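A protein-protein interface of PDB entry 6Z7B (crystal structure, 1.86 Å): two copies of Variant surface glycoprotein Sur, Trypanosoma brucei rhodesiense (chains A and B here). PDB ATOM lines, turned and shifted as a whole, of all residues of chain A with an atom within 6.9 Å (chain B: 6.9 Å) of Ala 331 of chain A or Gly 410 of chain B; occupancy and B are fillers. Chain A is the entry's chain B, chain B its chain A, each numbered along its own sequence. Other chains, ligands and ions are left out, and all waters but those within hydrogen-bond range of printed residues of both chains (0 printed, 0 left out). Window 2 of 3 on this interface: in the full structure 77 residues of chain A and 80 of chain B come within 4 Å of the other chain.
The side-chain carboxylate (OD2) of Asp 330 of chain A lies within hydrogen-bond range of the side-chain hydroxyl (OH) of Tyr 343 of chain A (2.7 Å). The side-chain hydroxyl of Tyr 407 of chain B lies within hydrogen-bond range of the side-chain amino group of Lys 411 of chain B.
Thr 93 of chain A touches Lys 409 of chain B (CG2 to CB, 3.9 Å). O of Ala 327 of chain A touches CD1 of Ile 383 of chain B, at 3.1 Å. Ala 327 of chain A touches Leu 403 of chain B. Ile 383 of chain B touches Asp 330 of chain A (CG1 to OD2, 3.5 Å). Ile 383 of chain B touches Ala 331 of chain A. Ala 331 of chain A touches Ala 406 of chain B (CB to O, 3.7 Å). Ala 331 of chain A touches Tyr 407 of chain B (CB to CA, 3.8 Å). O of Ala 331 of chain A touches CA of Gly 410 of chain B, 3.2 Å away. Leu 332 of chain A touches Ala 406 of chain B (CD2 to O, 3.6 Å). Lys 409 of chain B touches Leu 332 of chain A.
Ala 326 of chain A touches none of the printed residues of chain B. Printed residues of chain B within 4 Å of Asp 330 of chain A: Ile 383 (3.5 Å). Of chain B, only Ile 383, Ala 406, Tyr 407 and Gly 410 come within 4 Å of Ala 331 of chain A. Of the printed residues of chain A, Leu 403 of chain B touches Ala 327 (3.8 Å). Of the printed residues of chain A, Ala 406 of chain B touches Ala 331 and Leu 332. Of chain A, only Ala 331 and Leu 332 come within 4 Å of Gly 410 of chain B. The nearest residue of chain A that does not touch Gly 410 of chain B is Asn 90 of chain A (6.0 Å).
Of the 11 printed residues of chain B, 6 touch a printed residue of chain A. Hydrophobic or aromatic side chains of chain A within 4 Å of the printed part of chain B: Ala 327, Ala 331, Leu 332 and Tyr 343.
No position is printed for both chains.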
ATOM      1  N   ASN A  90      -0.104  -2.536  17.471  1.00  0.00           N
ATOM      2  CA  ASN A  90      -0.445  -3.948  17.383  1.00  0.00           C
ATOM      3  C   ASN A  90      -1.011  -4.454  18.692  1.00  0.00           C
ATOM      4  O   ASN A  90      -1.926  -5.283  18.698  1.00  0.00           O
ATOM      5  CB  ASN A  90       0.786  -4.758  16.990  1.00  0.00           C
ATOM      6  CG  ASN A  90       1.097  -4.636  15.541  1.00  0.00           C
ATOM      7  OD1 ASN A  90       0.180  -4.582  14.720  1.00  0.00           O
ATOM      8  ND2 ASN A  90       2.385  -4.566  15.199  1.00  0.00           N
ATOM      9  N   THR A  93      -4.608  -3.488  19.050  1.00  0.00           N
ATOM     10  CA  THR A  93      -5.451  -4.256  18.144  1.00  0.00           C
ATOM     11  C   THR A  93      -5.646  -5.681  18.640  1.00  0.00           C
ATOM     12  O   THR A  93      -6.670  -6.303  18.343  1.00  0.00           O
ATOM     13  CB  THR A  93      -4.862  -4.219  16.733  1.00  0.00           C
ATOM     14  OG1 THR A  93      -4.995  -2.892  16.216  1.00  0.00           O
ATOM     15  CG2 THR A  93      -5.587  -5.168  15.797  1.00  0.00           C
ATOM     16  N   MET A 325      -5.857 -15.648  23.278  1.00  0.00           N
ATOM     17  CA  MET A 325      -4.722 -14.790  22.975  1.00  0.00           C
ATOM     18  C   MET A 325      -3.573 -15.536  22.326  1.00  0.00           C
ATOM     19  O   MET A 325      -2.628 -14.890  21.864  1.00  0.00           O
ATOM     20  CB  MET A 325      -4.228 -14.101  24.245  1.00  0.00           C
ATOM     21  CG  MET A 325      -5.049 -12.892  24.634  1.00  0.00           C
ATOM     22  SD  MET A 325      -5.270 -11.740  23.269  1.00  0.00           S
ATOM     23  CE  MET A 325      -3.697 -10.913  23.225  1.00  0.00           C
ATOM     24  N   ALA A 326      -3.629 -16.868  22.278  1.00  0.00           N
ATOM     25  CA  ALA A 326      -2.630 -17.641  21.545  1.00  0.00           C
ATOM     26  C   ALA A 326      -2.701 -17.349  20.052  1.00  0.00           C
ATOM     27  O   ALA A 326      -1.723 -16.907  19.443  1.00  0.00           O
ATOM     28  CB  ALA A 326      -2.824 -19.135  21.812  1.00  0.00           C
ATOM     29  N   ALA A 327      -3.859 -17.592  19.440  1.00  0.00           N
ATOM     30  CA  ALA A 327      -3.999 -17.305  18.018  1.00  0.00           C
ATOM     31  C   ALA A 327      -3.946 -15.809  17.742  1.00  0.00           C
ATOM     32  O   ALA A 327      -3.388 -15.393  16.723  1.00  0.00           O
ATOM     33  CB  ALA A 327      -5.298 -17.908  17.481  1.00  0.00           C
ATOM     34  N   ILE A 328      -4.493 -14.989  18.638  1.00  0.00           N
ATOM     35  CA  ILE A 328      -4.542 -13.551  18.394  1.00  0.00           C
ATOM     36  C   ILE A 328      -3.149 -12.941  18.476  1.00  0.00           C
ATOM     37  O   ILE A 328      -2.823 -12.009  17.735  1.00  0.00           O
ATOM     38  CB  ILE A 328      -5.527 -12.881  19.374  1.00  0.00           C
ATOM     39  CG1 ILE A 328      -6.965 -13.123  18.903  1.00  0.00           C
ATOM     40  CG2 ILE A 328      -5.242 -11.374  19.488  1.00  0.00           C
ATOM     41  CD1 ILE A 328      -8.040 -12.680  19.858  1.00  0.00           C
ATOM     42  N   GLY A 329      -2.299 -13.455  19.362  1.00  0.00           N
ATOM     43  CA  GLY A 329      -0.926 -12.979  19.397  1.00  0.00           C
ATOM     44  C   GLY A 329      -0.116 -13.459  18.206  1.00  0.00           C
ATOM     45  O   GLY A 329       0.671 -12.701  17.628  1.00  0.00           O
ATOM     46  N   ASP A 330      -0.306 -14.724  17.820  1.00  0.00           N
ATOM     47  CA  ASP A 330       0.359 -15.281  16.646  1.00  0.00           C
ATOM     48  C   ASP A 330       0.021 -14.497  15.388  1.00  0.00           C
ATOM     49  O   ASP A 330       0.804 -14.476  14.435  1.00  0.00           O
ATOM     50  CB  ASP A 330      -0.044 -16.751  16.503  1.00  0.00           C
ATOM     51  CG  ASP A 330       0.551 -17.427  15.290  1.00  0.00           C
ATOM     52  OD1 ASP A 330       1.781 -17.371  15.102  1.00  0.00           O
ATOM     53  OD2 ASP A 330      -0.213 -18.065  14.544  1.00  0.00           O
ATOM     54  N   ALA A 331      -1.128 -13.841  15.361  1.00  0.00           N
ATOM     55  CA  ALA A 331      -1.522 -13.148  14.149  1.00  0.00           C
ATOM     56  C   ALA A 331      -0.989 -11.738  14.094  1.00  0.00           C
ATOM     57  O   ALA A 331      -0.773 -11.214  13.001  1.00  0.00           O
ATOM     58  CB  ALA A 331      -3.041 -13.118  14.016  1.00  0.00           C
ATOM     59  N   LEU A 332      -0.754 -11.114  15.245  1.00  0.00           N
ATOM     60  CA  LEU A 332      -0.355  -9.719  15.275  1.00  0.00           C
ATOM     61  C   LEU A 332       1.060  -9.500  15.763  1.00  0.00           C
ATOM     62  O   LEU A 332       1.633  -8.445  15.479  1.00  0.00           O
ATOM     63  CB  LEU A 332      -1.295  -8.908  16.170  1.00  0.00           C
ATOM     64  CG  LEU A 332      -2.705  -8.711  15.643  1.00  0.00           C
ATOM     65  CD1 LEU A 332      -3.636  -8.417  16.794  1.00  0.00           C
ATOM     66  CD2 LEU A 332      -2.725  -7.584  14.638  1.00  0.00           C
ATOM     67  N   LEU A 333       1.631 -10.454  16.495  1.00  0.00           N
ATOM     68  CA  LEU A 333       2.935 -10.256  17.106  1.00  0.00           C
ATOM     69  C   LEU A 333       4.057 -10.993  16.386  1.00  0.00           C
ATOM     70  O   LEU A 333       5.211 -10.554  16.469  1.00  0.00           O
ATOM     71  CB  LEU A 333       2.876 -10.665  18.581  1.00  0.00           C
ATOM     72  CG  LEU A 333       1.761  -9.963  19.370  1.00  0.00           C
ATOM     73  CD1 LEU A 333       1.823 -10.362  20.827  1.00  0.00           C
ATOM     74  CD2 LEU A 333       1.826  -8.440  19.224  1.00  0.00           C
ATOM     75  N   THR A 334       3.731 -12.105  15.717  1.00  0.00           N
ATOM     76  CA  THR A 334       4.489 -12.755  14.630  1.00  0.00           C
ATOM     77  C   THR A 334       3.873 -14.109  14.325  1.00  0.00           C
ATOM     78  O   THR A 334       4.208 -15.107  14.960  1.00  0.00           O
ATOM     79  CB  THR A 334       5.999 -12.978  14.920  1.00  0.00           C
ATOM     80  OG1 THR A 334       6.196 -13.296  16.303  1.00  0.00           O
ATOM     81  CG2 THR A 334       6.854 -11.786  14.473  1.00  0.00           C
ATOM     82  N   PRO A 337       2.412 -16.451  10.822  1.00  0.00           N
ATOM     83  CA  PRO A 337       1.455 -17.098  11.724  1.00  0.00           C
ATOM     84  C   PRO A 337       1.213 -18.553  11.349  1.00  0.00           C
ATOM     85  O   PRO A 337       0.725 -18.825  10.248  1.00  0.00           O
ATOM     86  CB  PRO A 337       0.182 -16.269  11.542  1.00  0.00           C
ATOM     87  CG  PRO A 337       0.330 -15.608  10.189  1.00  0.00           C
ATOM     88  CD  PRO A 337       1.734 -15.850   9.667  1.00  0.00           C
ATOM     89  N   TYR A 343      -0.470 -25.571  17.908  1.00  0.00           N
ATOM     90  CA  TYR A 343       0.751 -25.028  18.499  1.00  0.00           C
ATOM     91  C   TYR A 343       1.492 -26.064  19.352  1.00  0.00           C
ATOM     92  O   TYR A 343       0.944 -26.609  20.299  1.00  0.00           O
ATOM     93  CB  TYR A 343       0.437 -23.777  19.344  1.00  0.00           C
ATOM     94  CG  TYR A 343      -0.140 -22.623  18.545  1.00  0.00           C
ATOM     95  CD1 TYR A 343       0.303 -22.359  17.258  1.00  0.00           C
ATOM     96  CD2 TYR A 343      -1.129 -21.799  19.075  1.00  0.00           C
ATOM     97  CE1 TYR A 343      -0.220 -21.312  16.511  1.00  0.00           C
ATOM     98  CE2 TYR A 343      -1.661 -20.744  18.331  1.00  0.00           C
ATOM     99  CZ  TYR A 343      -1.199 -20.511  17.049  1.00  0.00           C
ATOM    100  OH  TYR A 343      -1.708 -19.474  16.292  1.00  0.00           O
ATOM    101  N   ALA B  81      -9.697  -3.471   7.581  1.00  0.00           N
ATOM    102  CA  ALA B  81      -8.488  -4.253   7.818  1.00  0.00           C
ATOM    103  C   ALA B  81      -8.044  -5.034   6.588  1.00  0.00           C
ATOM    104  O   ALA B  81      -6.870  -5.407   6.488  1.00  0.00           O
ATOM    105  CB  ALA B  81      -8.711  -5.215   8.987  1.00  0.00           C
ATOM    106  N   ILE B 383      -5.604 -20.298  11.070  1.00  0.00           N
ATOM    107  CA  ILE B 383      -4.462 -19.856  11.834  1.00  0.00           C
ATOM    108  C   ILE B 383      -3.915 -20.729  12.850  1.00  0.00           C
ATOM    109  O   ILE B 383      -2.802 -21.184  12.687  1.00  0.00           O
ATOM    110  CB  ILE B 383      -4.547 -18.392  12.342  1.00  0.00           C
ATOM    111  CG1 ILE B 383      -3.495 -18.093  13.427  1.00  0.00           C
ATOM    112  CG2 ILE B 383      -5.939 -18.028  12.761  1.00  0.00           C
ATOM    113  CD1 ILE B 383      -3.469 -16.687  13.909  1.00  0.00           C
ATOM    114  N   LEU B 403     -10.910 -13.054  15.931  1.00  0.00           N
ATOM    115  CA  LEU B 403      -9.752 -13.748  15.386  1.00  0.00           C
ATOM    116  C   LEU B 403      -9.508 -13.343  13.935  1.00  0.00           C
ATOM    117  O   LEU B 403      -8.355 -13.188  13.510  1.00  0.00           O
ATOM    118  CB  LEU B 403      -9.961 -15.258  15.524  1.00  0.00           C
ATOM    119  CG  LEU B 403      -8.937 -16.161  14.864  1.00  0.00           C
ATOM    120  CD1 LEU B 403      -7.545 -15.739  15.306  1.00  0.00           C
ATOM    121  CD2 LEU B 403      -9.226 -17.601  15.234  1.00  0.00           C
ATOM    122  N   ALA B 404     -10.585 -13.157  13.170  1.00  0.00           N
ATOM    123  CA  ALA B 404     -10.473 -12.651  11.808  1.00  0.00           C
ATOM    124  C   ALA B 404      -9.954 -11.222  11.768  1.00  0.00           C
ATOM    125  O   ALA B 404      -9.262 -10.845  10.820  1.00  0.00           O
ATOM    126  CB  ALA B 404     -11.833 -12.731  11.118  1.00  0.00           C
ATOM    127  N   LEU B 405     -10.285 -10.403  12.763  1.00  0.00           N
ATOM    128  CA  LEU B 405      -9.762  -9.042  12.772  1.00  0.00           C
ATOM    129  C   LEU B 405      -8.265  -9.035  13.053  1.00  0.00           C
ATOM    130  O   LEU B 405      -7.511  -8.279  12.427  1.00  0.00           O
ATOM    131  CB  LEU B 405     -10.508  -8.193  13.798  1.00  0.00           C
ATOM    132  CG  LEU B 405     -10.119  -6.721  13.783  1.00  0.00           C
ATOM    133  CD1 LEU B 405     -10.483  -6.113  12.448  1.00  0.00           C
ATOM    134  CD2 LEU B 405     -10.805  -5.984  14.929  1.00  0.00           C
ATOM    135  N   ALA B 406      -7.818  -9.873  13.990  1.00  0.00           N
ATOM    136  CA  ALA B 406      -6.395  -9.976  14.277  1.00  0.00           C
ATOM    137  C   ALA B 406      -5.630 -10.532  13.080  1.00  0.00           C
ATOM    138  O   ALA B 406      -4.542 -10.040  12.751  1.00  0.00           O
ATOM    139  CB  ALA B 406      -6.174 -10.847  15.515  1.00  0.00           C
ATOM    140  N   TYR B 407      -6.189 -11.544  12.406  1.00  0.00           N
ATOM    141  CA  TYR B 407      -5.502 -12.152  11.269  1.00  0.00           C
ATOM    142  C   TYR B 407      -5.216 -11.129  10.179  1.00  0.00           C
ATOM    143  O   TYR B 407      -4.094 -11.040   9.676  1.00  0.00           O
ATOM    144  CB  TYR B 407      -6.328 -13.302  10.701  1.00  0.00           C
ATOM    145  CG  TYR B 407      -5.688 -13.941   9.483  1.00  0.00           C
ATOM    146  CD1 TYR B 407      -4.684 -14.896   9.624  1.00  0.00           C
ATOM    147  CD2 TYR B 407      -6.075 -13.582   8.197  1.00  0.00           C
ATOM    148  CE1 TYR B 407      -4.083 -15.474   8.518  1.00  0.00           C
ATOM    149  CE2 TYR B 407      -5.485 -14.154   7.087  1.00  0.00           C
ATOM    150  CZ  TYR B 407      -4.489 -15.100   7.251  1.00  0.00           C
ATOM    151  OH  TYR B 407      -3.894 -15.665   6.143  1.00  0.00           O
ATOM    152  N   HIS B 408      -6.222 -10.350   9.797  1.00  0.00           N
ATOM    153  CA  HIS B 408      -6.052  -9.451   8.666  1.00  0.00           C
ATOM    154  C   HIS B 408      -5.321  -8.177   9.049  1.00  0.00           C
ATOM    155  O   HIS B 408      -4.580  -7.630   8.228  1.00  0.00           O
ATOM    156  CB  HIS B 408      -7.408  -9.144   8.038  1.00  0.00           C
ATOM    157  CG  HIS B 408      -7.920 -10.272   7.204  1.00  0.00           C
ATOM    158  ND1 HIS B 408      -7.562 -10.439   5.886  1.00  0.00           N
ATOM    159  CD2 HIS B 408      -8.703 -11.330   7.518  1.00  0.00           C
ATOM    160  CE1 HIS B 408      -8.128 -11.535   5.415  1.00  0.00           C
ATOM    161  NE2 HIS B 408      -8.821 -12.097   6.386  1.00  0.00           N
ATOM    162  N   LYS B 409      -5.482  -7.696  10.277  1.00  0.00           N
ATOM    163  CA  LYS B 409      -4.626  -6.599  10.692  1.00  0.00           C
ATOM    164  C   LYS B 409      -3.175  -7.043  10.792  1.00  0.00           C
ATOM    165  O   LYS B 409      -2.278  -6.196  10.745  1.00  0.00           O
ATOM    166  CB  LYS B 409      -5.112  -6.004  12.019  1.00  0.00           C
ATOM    167  CG  LYS B 409      -6.375  -5.167  11.903  1.00  0.00           C
ATOM    168  CD  LYS B 409      -6.119  -3.854  11.190  1.00  0.00           C
ATOM    169  CE  LYS B 409      -5.639  -2.785  12.139  1.00  0.00           C
ATOM    170  NZ  LYS B 409      -5.486  -1.473  11.445  1.00  0.00           N
ATOM    171  N   GLY B 410      -2.928  -8.354  10.888  1.00  0.00           N
ATOM    172  CA  GLY B 410      -1.575  -8.880  10.926  1.00  0.00           C
ATOM    173  C   GLY B 410      -0.860  -8.953   9.587  1.00  0.00           C
ATOM    174  O   GLY B 410       0.369  -9.055   9.566  1.00  0.00           O
ATOM    175  N   LYS B 411      -1.586  -8.902   8.474  1.00  0.00           N
ATOM    176  CA  LYS B 411      -0.955  -8.856   7.154  1.00  0.00           C
ATOM    177  C   LYS B 411      -0.938  -7.439   6.598  1.00  0.00           C
ATOM    178  O   LYS B 411      -1.918  -6.707   6.724  1.00  0.00           O
ATOM    179  CB  LYS B 411      -1.681  -9.775   6.178  1.00  0.00           C
ATOM    180  CG  LYS B 411      -2.462 -10.873   6.850  1.00  0.00           C
ATOM    181  CD  LYS B 411      -3.311 -11.598   5.842  1.00  0.00           C
ATOM    182  CE  LYS B 411      -2.432 -12.269   4.815  1.00  0.00           C
ATOM    183  NZ  LYS B 411      -3.204 -13.170   3.918  1.00  0.00           N
